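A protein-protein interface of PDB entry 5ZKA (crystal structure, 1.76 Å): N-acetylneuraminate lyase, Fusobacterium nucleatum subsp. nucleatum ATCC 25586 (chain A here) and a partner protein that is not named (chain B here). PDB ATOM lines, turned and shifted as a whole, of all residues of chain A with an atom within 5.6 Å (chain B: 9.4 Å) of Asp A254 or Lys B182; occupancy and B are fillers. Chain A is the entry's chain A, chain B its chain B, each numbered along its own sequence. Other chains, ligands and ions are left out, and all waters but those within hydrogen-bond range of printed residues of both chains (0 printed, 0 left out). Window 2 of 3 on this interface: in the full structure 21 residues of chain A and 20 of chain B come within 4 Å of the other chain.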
ATOM      1  N   GLN A 249     -12.117  -7.338  11.184  1.00  0.00           N
ATOM      2  CA  GLN A 249     -12.152  -6.301  12.220  1.00  0.00           C
ATOM      3  C   GLN A 249     -13.561  -5.743  12.389  1.00  0.00           C
ATOM      4  O   GLN A 249     -13.988  -5.439  13.512  1.00  0.00           O
ATOM      5  CB  GLN A 249     -11.177  -5.173  11.891  1.00  0.00           C
ATOM      6  CG  GLN A 249     -11.070  -4.105  12.983  1.00  0.00           C
ATOM      7  CD  GLN A 249     -10.207  -4.582  14.133  1.00  0.00           C
ATOM      8  OE1 GLN A 249      -8.999  -4.725  13.974  1.00  0.00           O
ATOM      9  NE2 GLN A 249     -10.824  -4.858  15.283  1.00  0.00           N
ATOM     10  N   HIS A 250     -14.297  -5.598  11.279  1.00  0.00           N
ATOM     11  CA  HIS A 250     -15.675  -5.124  11.358  1.00  0.00           C
ATOM     12  C   HIS A 250     -16.535  -6.085  12.171  1.00  0.00           C
ATOM     13  O   HIS A 250     -17.334  -5.664  13.014  1.00  0.00           O
ATOM     14  CB  HIS A 250     -16.257  -4.971   9.953  1.00  0.00           C
ATOM     15  CG  HIS A 250     -15.919  -3.677   9.268  1.00  0.00           C
ATOM     16  ND1 HIS A 250     -15.762  -2.485   9.941  1.00  0.00           N
ATOM     17  CD2 HIS A 250     -15.786  -3.386   7.951  1.00  0.00           C
ATOM     18  CE1 HIS A 250     -15.516  -1.520   9.068  1.00  0.00           C
ATOM     19  NE2 HIS A 250     -15.524  -2.041   7.853  1.00  0.00           N
ATOM     20  N   THR A 251     -16.427  -7.384  11.885  1.00  0.00           N
ATOM     21  CA  THR A 251     -17.218  -8.366  12.616  1.00  0.00           C
ATOM     22  C   THR A 251     -16.810  -8.391  14.081  1.00  0.00           C
ATOM     23  O   THR A 251     -17.666  -8.423  14.976  1.00  0.00           O
ATOM     24  CB  THR A 251     -17.036  -9.748  11.985  1.00  0.00           C
ATOM     25  OG1 THR A 251     -17.549  -9.735  10.640  1.00  0.00           O
ATOM     26  CG2 THR A 251     -17.771 -10.812  12.793  1.00  0.00           C
ATOM     27  N   THR A 252     -15.501  -8.365  14.332  1.00  0.00           N
ATOM     28  CA  THR A 252     -14.982  -8.315  15.700  1.00  0.00           C
ATOM     29  C   THR A 252     -15.536  -7.119  16.463  1.00  0.00           C
ATOM     30  O   THR A 252     -15.944  -7.240  17.627  1.00  0.00           O
ATOM     31  CB  THR A 252     -13.456  -8.271  15.660  1.00  0.00           C
ATOM     32  OG1 THR A 252     -12.962  -9.562  15.279  1.00  0.00           O
ATOM     33  CG2 THR A 252     -12.851  -7.887  17.027  1.00  0.00           C
ATOM     34  N   ASN A 253     -15.585  -5.953  15.822  1.00  0.00           N
ATOM     35  CA  ASN A 253     -16.042  -4.777  16.546  1.00  0.00           C
ATOM     36  C   ASN A 253     -17.555  -4.743  16.742  1.00  0.00           C
ATOM     37  O   ASN A 253     -18.025  -4.065  17.659  1.00  0.00           O
ATOM     38  CB  ASN A 253     -15.529  -3.505  15.848  1.00  0.00           C
ATOM     39  CG  ASN A 253     -14.049  -3.270  16.119  1.00  0.00           C
ATOM     40  OD1 ASN A 253     -13.386  -4.128  16.702  1.00  0.00           O
ATOM     41  ND2 ASN A 253     -13.526  -2.111  15.709  1.00  0.00           N
ATOM     42  N   ASP A 254     -18.333  -5.461  15.929  1.00  0.00           N
ATOM     43  CA  ASP A 254     -19.733  -5.681  16.294  1.00  0.00           C
ATOM     44  C   ASP A 254     -19.822  -6.461  17.602  1.00  0.00           C
ATOM     45  O   ASP A 254     -20.655  -6.169  18.469  1.00  0.00           O
ATOM     46  CB  ASP A 254     -20.458  -6.452  15.187  1.00  0.00           C
ATOM     47  CG  ASP A 254     -20.849  -5.585  13.998  1.00  0.00           C
ATOM     48  OD1 ASP A 254     -20.740  -4.337  14.077  1.00  0.00           O
ATOM     49  OD2 ASP A 254     -21.287  -6.170  12.982  1.00  0.00           O
ATOM     50  N   LEU A 255     -18.978  -7.478  17.747  1.00  0.00           N
ATOM     51  CA  LEU A 255     -18.946  -8.245  18.984  1.00  0.00           C
ATOM     52  C   LEU A 255     -18.437  -7.388  20.142  1.00  0.00           C
ATOM     53  O   LEU A 255     -19.041  -7.364  21.220  1.00  0.00           O
ATOM     54  CB  LEU A 255     -18.077  -9.487  18.793  1.00  0.00           C
ATOM     55  CG  LEU A 255     -17.686 -10.225  20.075  1.00  0.00           C
ATOM     56  CD1 LEU A 255     -18.930 -10.785  20.780  1.00  0.00           C
ATOM     57  CD2 LEU A 255     -16.693 -11.332  19.748  1.00  0.00           C
ATOM     58  N   ILE A 256     -17.338  -6.663  19.934  1.00  0.00           N
ATOM     59  CA  ILE A 256     -16.788  -5.836  21.011  1.00  0.00           C
ATOM     60  C   ILE A 256     -17.782  -4.756  21.416  1.00  0.00           C
ATOM     61  O   ILE A 256     -17.936  -4.445  22.603  1.00  0.00           O
ATOM     62  CB  ILE A 256     -15.428  -5.245  20.589  1.00  0.00           C
ATOM     63  CG1 ILE A 256     -14.391  -6.373  20.489  1.00  0.00           C
ATOM     64  CG2 ILE A 256     -14.965  -4.172  21.590  1.00  0.00           C
ATOM     65  CD1 ILE A 256     -13.003  -5.895  20.092  1.00  0.00           C
ATOM     66  N   GLU A 257     -18.488  -4.176  20.443  1.00  0.00           N
ATOM     67  CA  GLU A 257     -19.466  -3.146  20.772  1.00  0.00           C
ATOM     68  C   GLU A 257     -20.548  -3.700  21.687  1.00  0.00           C
ATOM     69  O   GLU A 257     -20.961  -3.035  22.646  1.00  0.00           O
ATOM     70  CB  GLU A 257     -20.077  -2.582  19.488  1.00  0.00           C
ATOM     71  CG  GLU A 257     -21.197  -1.593  19.688  1.00  0.00           C
ATOM     72  CD  GLU A 257     -21.903  -1.288  18.372  1.00  0.00           C
ATOM     73  OE1 GLU A 257     -21.407  -0.425  17.627  1.00  0.00           O
ATOM     74  OE2 GLU A 257     -22.934  -1.933  18.073  1.00  0.00           O
ATOM     75  N   GLY A 258     -20.990  -4.938  21.435  1.00  0.00           N
ATOM     76  CA  GLY A 258     -21.951  -5.560  22.333  1.00  0.00           C
ATOM     77  C   GLY A 258     -21.353  -5.891  23.689  1.00  0.00           C
ATOM     78  O   GLY A 258     -21.999  -5.709  24.725  1.00  0.00           O
ATOM     79  N   ILE A 259     -20.117  -6.393  23.701  1.00  0.00           N
ATOM     80  CA  ILE A 259     -19.452  -6.702  24.964  1.00  0.00           C
ATOM     81  C   ILE A 259     -19.377  -5.455  25.829  1.00  0.00           C
ATOM     82  O   ILE A 259     -19.724  -5.473  27.017  1.00  0.00           O
ATOM     83  CB  ILE A 259     -18.053  -7.289  24.700  1.00  0.00           C
ATOM     84  CG1 ILE A 259     -18.145  -8.688  24.078  1.00  0.00           C
ATOM     85  CG2 ILE A 259     -17.203  -7.276  25.971  1.00  0.00           C
ATOM     86  CD1 ILE A 259     -16.798  -9.218  23.624  1.00  0.00           C
ATOM     87  N   LEU A 300     -24.984 -12.670  21.778  1.00  0.00           N
ATOM     88  CA  LEU A 300     -23.653 -12.416  21.224  1.00  0.00           C
ATOM     89  C   LEU A 300     -22.923 -13.722  20.934  1.00  0.00           C
ATOM     90  O   LEU A 300     -22.271 -13.867  19.891  1.00  0.00           O
ATOM     91  CB  LEU A 300     -22.815 -11.574  22.192  1.00  0.00           C
ATOM     92  CG  LEU A 300     -23.247 -10.132  22.455  1.00  0.00           C
ATOM     93  CD1 LEU A 300     -22.390  -9.510  23.564  1.00  0.00           C
ATOM     94  CD2 LEU A 300     -23.150  -9.307  21.183  1.00  0.00           C
ATOM     95  N   PHE A 304     -21.878 -14.627  17.113  1.00  0.00           N
ATOM     96  CA  PHE A 304     -20.481 -14.374  16.771  1.00  0.00           C
ATOM     97  C   PHE A 304     -19.532 -15.533  17.056  1.00  0.00           C
ATOM     98  O   PHE A 304     -18.464 -15.588  16.436  1.00  0.00           O
ATOM     99  CB  PHE A 304     -19.973 -13.112  17.498  1.00  0.00           C
ATOM    100  CG  PHE A 304     -20.640 -11.843  17.027  1.00  0.00           C
ATOM    101  CD1 PHE A 304     -20.382 -11.338  15.759  1.00  0.00           C
ATOM    102  CD2 PHE A 304     -21.564 -11.191  17.821  1.00  0.00           C
ATOM    103  CE1 PHE A 304     -21.008 -10.190  15.312  1.00  0.00           C
ATOM    104  CE2 PHE A 304     -22.184 -10.027  17.384  1.00  0.00           C
ATOM    105  CZ  PHE A 304     -21.911  -9.531  16.128  1.00  0.00           C
ATOM    106  N   LEU B   1     -21.840   0.408  -0.802  1.00  0.00           N
ATOM    107  CA  LEU B   1     -23.008   0.421  -1.675  1.00  0.00           C
ATOM    108  C   LEU B   1     -22.734   1.233  -2.946  1.00  0.00           C
ATOM    109  O   LEU B   1     -21.912   2.145  -2.946  1.00  0.00           O
ATOM    110  CB  LEU B   1     -24.224   0.974  -0.925  1.00  0.00           C
ATOM    111  CG  LEU B   1     -25.543   1.004  -1.702  1.00  0.00           C
ATOM    112  CD1 LEU B   1     -26.705   0.485  -0.876  1.00  0.00           C
ATOM    113  CD2 LEU B   1     -25.822   2.407  -2.152  1.00  0.00           C
ATOM    114  N   LEU B 152     -22.496   7.776  17.426  1.00  0.00           N
ATOM    115  CA  LEU B 152     -22.855   6.998  16.249  1.00  0.00           C
ATOM    116  C   LEU B 152     -24.295   7.267  15.829  1.00  0.00           C
ATOM    117  O   LEU B 152     -24.591   7.382  14.634  1.00  0.00           O
ATOM    118  CB  LEU B 152     -22.626   5.511  16.536  1.00  0.00           C
ATOM    119  CG  LEU B 152     -22.323   4.488  15.437  1.00  0.00           C
ATOM    120  CD1 LEU B 152     -21.450   5.046  14.342  1.00  0.00           C
ATOM    121  CD2 LEU B 152     -21.645   3.288  16.065  1.00  0.00           C
ATOM    122  N   PHE B 159     -26.822  11.592   8.621  1.00  0.00           N
ATOM    123  CA  PHE B 159     -26.713  10.807   7.393  1.00  0.00           C
ATOM    124  C   PHE B 159     -28.057  10.319   6.881  1.00  0.00           C
ATOM    125  O   PHE B 159     -28.105   9.738   5.792  1.00  0.00           O
ATOM    126  CB  PHE B 159     -25.777   9.616   7.604  1.00  0.00           C
ATOM    127  CG  PHE B 159     -24.327   9.980   7.536  1.00  0.00           C
ATOM    128  CD1 PHE B 159     -23.886  10.962   6.659  1.00  0.00           C
ATOM    129  CD2 PHE B 159     -23.399   9.360   8.366  1.00  0.00           C
ATOM    130  CE1 PHE B 159     -22.544  11.313   6.607  1.00  0.00           C
ATOM    131  CE2 PHE B 159     -22.064   9.699   8.314  1.00  0.00           C
ATOM    132  CZ  PHE B 159     -21.629  10.671   7.434  1.00  0.00           C
ATOM    133  N   PHE B 174      -9.914   5.827  16.335  1.00  0.00           N
ATOM    134  CA  PHE B 174      -9.982   4.847  15.253  1.00  0.00           C
ATOM    135  C   PHE B 174     -11.012   3.748  15.496  1.00  0.00           C
ATOM    136  O   PHE B 174     -11.369   3.036  14.550  1.00  0.00           O
ATOM    137  CB  PHE B 174      -8.578   4.278  14.996  1.00  0.00           C
ATOM    138  CG  PHE B 174      -7.691   5.248  14.272  1.00  0.00           C
ATOM    139  CD1 PHE B 174      -7.101   6.300  14.954  1.00  0.00           C
ATOM    140  CD2 PHE B 174      -7.494   5.150  12.912  1.00  0.00           C
ATOM    141  CE1 PHE B 174      -6.318   7.229  14.296  1.00  0.00           C
ATOM    142  CE2 PHE B 174      -6.708   6.088  12.235  1.00  0.00           C
ATOM    143  CZ  PHE B 174      -6.122   7.128  12.939  1.00  0.00           C
ATOM    144  N   TYR B 175     -11.514   3.605  16.722  1.00  0.00           N
ATOM    145  CA  TYR B 175     -12.667   2.743  16.942  1.00  0.00           C
ATOM    146  C   TYR B 175     -13.920   3.381  16.350  1.00  0.00           C
ATOM    147  O   TYR B 175     -14.644   2.752  15.570  1.00  0.00           O
ATOM    148  CB  TYR B 175     -12.823   2.478  18.439  1.00  0.00           C
ATOM    149  CG  TYR B 175     -14.015   1.645  18.833  1.00  0.00           C
ATOM    150  CD1 TYR B 175     -14.419   0.547  18.073  1.00  0.00           C
ATOM    151  CD2 TYR B 175     -14.738   1.951  19.979  1.00  0.00           C
ATOM    152  CE1 TYR B 175     -15.525  -0.215  18.444  1.00  0.00           C
ATOM    153  CE2 TYR B 175     -15.835   1.199  20.355  1.00  0.00           C
ATOM    154  CZ  TYR B 175     -16.227   0.118  19.578  1.00  0.00           C
ATOM    155  OH  TYR B 175     -17.320  -0.621  19.959  1.00  0.00           O
ATOM    156  N   LEU B 176     -14.172   4.653  16.683  1.00  0.00           N
ATOM    157  CA  LEU B 176     -15.308   5.356  16.090  1.00  0.00           C
ATOM    158  C   LEU B 176     -15.200   5.392  14.571  1.00  0.00           C
ATOM    159  O   LEU B 176     -16.203   5.228  13.867  1.00  0.00           O
ATOM    160  CB  LEU B 176     -15.408   6.779  16.652  1.00  0.00           C
ATOM    161  CG  LEU B 176     -16.570   7.628  16.111  1.00  0.00           C
ATOM    162  CD1 LEU B 176     -17.917   6.983  16.451  1.00  0.00           C
ATOM    163  CD2 LEU B 176     -16.518   9.050  16.645  1.00  0.00           C
ATOM    164  N   LEU B 177     -13.993   5.608  14.044  1.00  0.00           N
ATOM    165  CA  LEU B 177     -13.819   5.665  12.595  1.00  0.00           C
ATOM    166  C   LEU B 177     -14.221   4.343  11.943  1.00  0.00           C
ATOM    167  O   LEU B 177     -14.896   4.328  10.907  1.00  0.00           O
ATOM    168  CB  LEU B 177     -12.366   6.018  12.262  1.00  0.00           C
ATOM    169  CG  LEU B 177     -11.959   6.173  10.798  1.00  0.00           C
ATOM    170  CD1 LEU B 177     -12.709   7.341  10.161  1.00  0.00           C
ATOM    171  CD2 LEU B 177     -10.440   6.387  10.676  1.00  0.00           C
ATOM    172  N   GLU B 178     -13.829   3.218  12.553  1.00  0.00           N
ATOM    173  CA  GLU B 178     -14.255   1.914  12.058  1.00  0.00           C
ATOM    174  C   GLU B 178     -15.770   1.757  12.140  1.00  0.00           C
ATOM    175  O   GLU B 178     -16.411   1.244  11.206  1.00  0.00           O
ATOM    176  CB  GLU B 178     -13.548   0.814  12.862  1.00  0.00           C
ATOM    177  CG  GLU B 178     -13.933  -0.599  12.439  1.00  0.00           C
ATOM    178  CD  GLU B 178     -15.186  -1.071  13.132  1.00  0.00           C
ATOM    179  OE1 GLU B 178     -15.400  -0.652  14.289  1.00  0.00           O
ATOM    180  OE2 GLU B 178     -15.963  -1.831  12.515  1.00  0.00           O
ATOM    181  N   ARG B 179     -16.357   2.170  13.266  1.00  0.00           N
ATOM    182  CA  ARG B 179     -17.793   2.024  13.456  1.00  0.00           C
ATOM    183  C   ARG B 179     -18.566   2.840  12.432  1.00  0.00           C
ATOM    184  O   ARG B 179     -19.558   2.363  11.870  1.00  0.00           O
ATOM    185  CB  ARG B 179     -18.178   2.438  14.878  1.00  0.00           C
ATOM    186  CG  ARG B 179     -17.627   1.518  16.001  1.00  0.00           C
ATOM    187  CD  ARG B 179     -18.473   0.251  16.165  1.00  0.00           C
ATOM    188  NE  ARG B 179     -18.079  -0.746  15.167  1.00  0.00           N
ATOM    189  CZ  ARG B 179     -18.791  -1.815  14.827  1.00  0.00           C
ATOM    190  NH1 ARG B 179     -19.963  -2.068  15.406  1.00  0.00           N
ATOM    191  NH2 ARG B 179     -18.322  -2.633  13.899  1.00  0.00           N
ATOM    192  N   VAL B 180     -18.119   4.073  12.170  1.00  0.00           N
ATOM    193  CA  VAL B 180     -18.781   4.912  11.170  1.00  0.00           C
ATOM    194  C   VAL B 180     -18.630   4.301   9.778  1.00  0.00           C
ATOM    195  O   VAL B 180     -19.578   4.285   8.989  1.00  0.00           O
ATOM    196  CB  VAL B 180     -18.230   6.348  11.234  1.00  0.00           C
ATOM    197  CG1 VAL B 180     -18.808   7.219  10.091  1.00  0.00           C
ATOM    198  CG2 VAL B 180     -18.521   6.987  12.610  1.00  0.00           C
ATOM    199  N   ARG B 181     -17.441   3.784   9.451  1.00  0.00           N
ATOM    200  CA  ARG B 181     -17.241   3.167   8.143  1.00  0.00           C
ATOM    201  C   ARG B 181     -18.172   1.975   7.936  1.00  0.00           C
ATOM    202  O   ARG B 181     -18.751   1.801   6.853  1.00  0.00           O
ATOM    203  CB  ARG B 181     -15.778   2.744   7.992  1.00  0.00           C
ATOM    204  CG  ARG B 181     -15.475   1.807   6.840  1.00  0.00           C
ATOM    205  CD  ARG B 181     -15.395   2.546   5.492  1.00  0.00           C
ATOM    206  NE  ARG B 181     -16.665   3.188   5.163  1.00  0.00           N
ATOM    207  CZ  ARG B 181     -16.813   4.209   4.319  1.00  0.00           C
ATOM    208  NH1 ARG B 181     -15.768   4.723   3.679  1.00  0.00           N
ATOM    209  NH2 ARG B 181     -18.022   4.713   4.111  1.00  0.00           N
ATOM    210  N   LYS B 182     -18.329   1.143   8.970  1.00  0.00           N
ATOM    211  CA  LYS B 182     -19.188  -0.028   8.855  1.00  0.00           C
ATOM    212  C   LYS B 182     -20.656   0.373   8.763  1.00  0.00           C
ATOM    213  O   LYS B 182     -21.413  -0.194   7.969  1.00  0.00           O
ATOM    214  CB  LYS B 182     -18.955  -0.953  10.053  1.00  0.00           C
ATOM    215  CG  LYS B 182     -20.060  -1.996  10.241  1.00  0.00           C
ATOM    216  CD  LYS B 182     -19.500  -3.331  10.659  1.00  0.00           C
ATOM    217  CE  LYS B 182     -20.547  -4.426  10.545  1.00  0.00           C
ATOM    218  NZ  LYS B 182     -21.778  -4.085  11.320  1.00  0.00           N
ATOM    219  N   ALA B 183     -21.070   1.360   9.561  1.00  0.00           N
ATOM    220  CA  ALA B 183     -22.479   1.730   9.641  1.00  0.00           C
ATOM    221  C   ALA B 183     -22.953   2.512   8.421  1.00  0.00           C
ATOM    222  O   ALA B 183     -24.153   2.511   8.122  1.00  0.00           O
ATOM    223  CB  ALA B 183     -22.736   2.545  10.907  1.00  0.00           C
ATOM    224  N   PHE B 184     -22.056   3.200   7.720  1.00  0.00           N
ATOM    225  CA  PHE B 184     -22.437   4.049   6.585  1.00  0.00           C
ATOM    226  C   PHE B 184     -21.543   3.759   5.387  1.00  0.00           C
ATOM    227  O   PHE B 184     -20.734   4.599   4.977  1.00  0.00           O
ATOM    228  CB  PHE B 184     -22.384   5.524   6.980  1.00  0.00           C
ATOM    229  CG  PHE B 184     -23.097   5.813   8.269  1.00  0.00           C
ATOM    230  CD1 PHE B 184     -24.480   5.865   8.309  1.00  0.00           C
ATOM    231  CD2 PHE B 184     -22.391   6.026   9.437  1.00  0.00           C
ATOM    232  CE1 PHE B 184     -25.144   6.116   9.497  1.00  0.00           C
ATOM    233  CE2 PHE B 184     -23.048   6.280  10.628  1.00  0.00           C
ATOM    234  CZ  PHE B 184     -24.426   6.320  10.660  1.00  0.00           C
ATOM    235  N   PRO B 185     -21.693   2.579   4.773  1.00  0.00           N
ATOM    236  CA  PRO B 185     -20.846   2.253   3.615  1.00  0.00           C
ATOM    237  C   PRO B 185     -21.148   3.103   2.387  1.00  0.00           C
ATOM    238  O   PRO B 185     -20.318   3.152   1.470  1.00  0.00           O
ATOM    239  CB  PRO B 185     -21.143   0.765   3.372  1.00  0.00           C
ATOM    240  CG  PRO B 185     -22.522   0.574   3.928  1.00  0.00           C
ATOM    241  CD  PRO B 185     -22.600   1.473   5.128  1.00  0.00           C
ATOM    242  N   ASP B 186     -22.281   3.800   2.360  1.00  0.00           N
ATOM    243  CA  ASP B 186     -22.685   4.635   1.230  1.00  0.00           C
ATOM    244  C   ASP B 186     -22.250   6.092   1.368  1.00  0.00           C
ATOM    245  O   ASP B 186     -22.514   6.885   0.456  1.00  0.00           O
ATOM    246  CB  ASP B 186     -24.208   4.582   1.065  1.00  0.00           C
ATOM    247  CG  ASP B 186     -24.938   5.040   2.323  1.00  0.00           C
ATOM    248  OD1 ASP B 186     -24.505   4.652   3.435  1.00  0.00           O
ATOM    249  OD2 ASP B 186     -25.933   5.792   2.205  1.00  0.00           O
ATOM    250  N   LYS B 187     -21.600   6.459   2.474  1.00  0.00           N
ATOM    251  CA  LYS B 187     -21.136   7.814   2.738  1.00  0.00           C
ATOM    252  C   LYS B 187     -19.629   7.899   2.547  1.00  0.00           C
ATOM    253  O   LYS B 187     -18.913   6.904   2.623  1.00  0.00           O
ATOM    254  CB  LYS B 187     -21.494   8.243   4.170  1.00  0.00           C
ATOM    255  CG  LYS B 187     -22.988   8.206   4.471  1.00  0.00           C
ATOM    256  CD  LYS B 187     -23.751   9.212   3.611  1.00  0.00           C
ATOM    257  CE  LYS B 187     -25.263   9.071   3.831  1.00  0.00           C
ATOM    258  NZ  LYS B 187     -26.070   9.966   2.936  1.00  0.00           N
ATOM    259  N   ILE B 189     -15.961   9.123   3.839  1.00  0.00           N
ATOM    260  CA  ILE B 189     -15.206   9.500   5.032  1.00  0.00           C
ATOM    261  C   ILE B 189     -13.838  10.002   4.595  1.00  0.00           C
ATOM    262  O   ILE B 189     -13.105   9.293   3.897  1.00  0.00           O
ATOM    263  CB  ILE B 189     -15.057   8.322   6.013  1.00  0.00           C
ATOM    264  CG1 ILE B 189     -16.419   7.681   6.277  1.00  0.00           C
ATOM    265  CG2 ILE B 189     -14.377   8.805   7.298  1.00  0.00           C
ATOM    266  CD1 ILE B 189     -16.348   6.359   7.073  1.00  0.00           C
ATOM    267  N   LEU B 203      -8.668   1.355   7.283  1.00  0.00           N
ATOM    268  CA  LEU B 203     -10.039   1.268   7.766  1.00  0.00           C
ATOM    269  C   LEU B 203     -11.049   1.717   6.724  1.00  0.00           C
ATOM    270  O   LEU B 203     -12.231   1.874   7.056  1.00  0.00           O
ATOM    271  CB  LEU B 203     -10.226   2.095   9.037  1.00  0.00           C
ATOM    272  CG  LEU B 203      -9.560   1.468  10.269  1.00  0.00           C
ATOM    273  CD1 LEU B 203      -9.708   2.387  11.462  1.00  0.00           C
ATOM    274  CD2 LEU B 203     -10.183   0.088  10.566  1.00  0.00           C
ATOM    275  N   GLY B 204     -10.613   1.941   5.484  1.00  0.00           N
ATOM    276  CA  GLY B 204     -11.543   2.183   4.390  1.00  0.00           C
ATOM    277  C   GLY B 204     -11.957   3.624   4.165  1.00  0.00           C
ATOM    278  O   GLY B 204     -12.980   3.860   3.500  1.00  0.00           O
ATOM    279  N   VAL B 205     -11.192   4.601   4.657  1.00  0.00           N
ATOM    280  CA  VAL B 205     -11.552   5.981   4.359  1.00  0.00           C
ATOM    281  C   VAL B 205     -11.436   6.207   2.866  1.00  0.00           C
ATOM    282  O   VAL B 205     -10.688   5.525   2.150  1.00  0.00           O
ATOM    283  CB  VAL B 205     -10.717   7.025   5.123  1.00  0.00           C
ATOM    284  CG1 VAL B 205     -10.824   6.788   6.606  1.00  0.00           C
ATOM    285  CG2 VAL B 205      -9.268   7.009   4.668  1.00  0.00           C
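The side-chain amide nitrogen (NE2) of Gln A249 is in hydrogen-bond range of the side-chain amide oxygen (OD1) of Asn A253 (3.0 Å).
The side-chain carboxylate of Glu B178 is in salt-bridge range of the guanidinium group of Arg B179 (2.8 Å).
NH2 of Arg B181 is in hydrogen-bond range of O of Phe B184, 2.8 Å away.
The backbone carbonyl oxygen (O) of Lys B187 lies within hydrogen-bond range of the guanidinium group (NH2) of Arg B181.
O of Gly B204 sits at hydrogen-bond distance from NH1 of Arg B181, at 2.9 Å.
Of the 13 printed residues of chain A, 4 touch a printed residue of chain B.
Hydrophobic or aromatic side chains of chain A that line the printed part of chain B: His A250.
Among the printed residues, Asp or Glu carboxylates within 4 Å of a Lys or Arg side-chain nitrogen of the other chain: Asp A254 with Arg B179, Asp A254 with Lys B182 and Glu A257 with Arg B179.
Of the printed residues of chain B, Asn A253 touches Tyr B175 (3.7 Å), Glu B178 (2.8 Å) and Arg B179 (3.5 Å).
Of chain B, only Arg B179 and Lys B182 come within 4 Å of Asp A254.
Of chain B, only Tyr B175 (3.4 Å) and Arg B179 (3.1 Å) come within 4 Å of Glu A257.
Gly A258 touches none of the printed residues of chain B.
Printed residues of chain A within 4 Å of Tyr B175: Asn A253 and Glu A257.
Of the printed residues of chain A, Glu B178 touches His A250 (2.7 Å) and Asn A253 (2.8 Å).
Of the printed residues of chain A, Arg B179 touches His A250 (3.3 Å), Asn A253 (3.5 Å), Asp A254 (2.7 Å) and Glu A257 (3.1 Å).
Of chain A, only His A250 (3.5 Å) and Asp A254 (2.7 Å) come within 4 Å of Lys B182.
The nearest residue of chain B that does not touch Asp A254 is Glu B178 (5.5 Å).
The side-chain carboxylate (OE2) of Glu B178 is in hydrogen-bond range of a ring nitrogen (ND1) of His A250 (2.7 Å).
The guanidinium group (NH2) of Arg B179 is in hydrogen-bond range of the backbone carbonyl oxygen (O) of His A250, 3.3 Å away.
OE1 of Glu B178 lies within hydrogen-bond range of ND2 of Asn A253, at 2.8 Å.
The guanidinium group (NH1) of Arg B179 is in salt-bridge range of the side-chain carboxylate (OD1) of Asp A254, at 2.7 Å.
OD2 of Asp A254 lies within salt-bridge range of NZ of Lys B182, at 2.7 Å.
The side-chain carboxylate (OE1) of Glu A257 lies within salt-bridge range of the guanidinium group (NH1) of Arg B179 (3.1 Å).
Among the printed residues, merely in contact across the chains: His A250 with Arg B181 (3.98 Å), His A250 with Lys B182 (3.5 Å), Asn A253 with Tyr B175 (3.7 Å), Asn A253 with Arg B179 (3.5 Å) and Glu A257 with Tyr B175 (3.4 Å).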
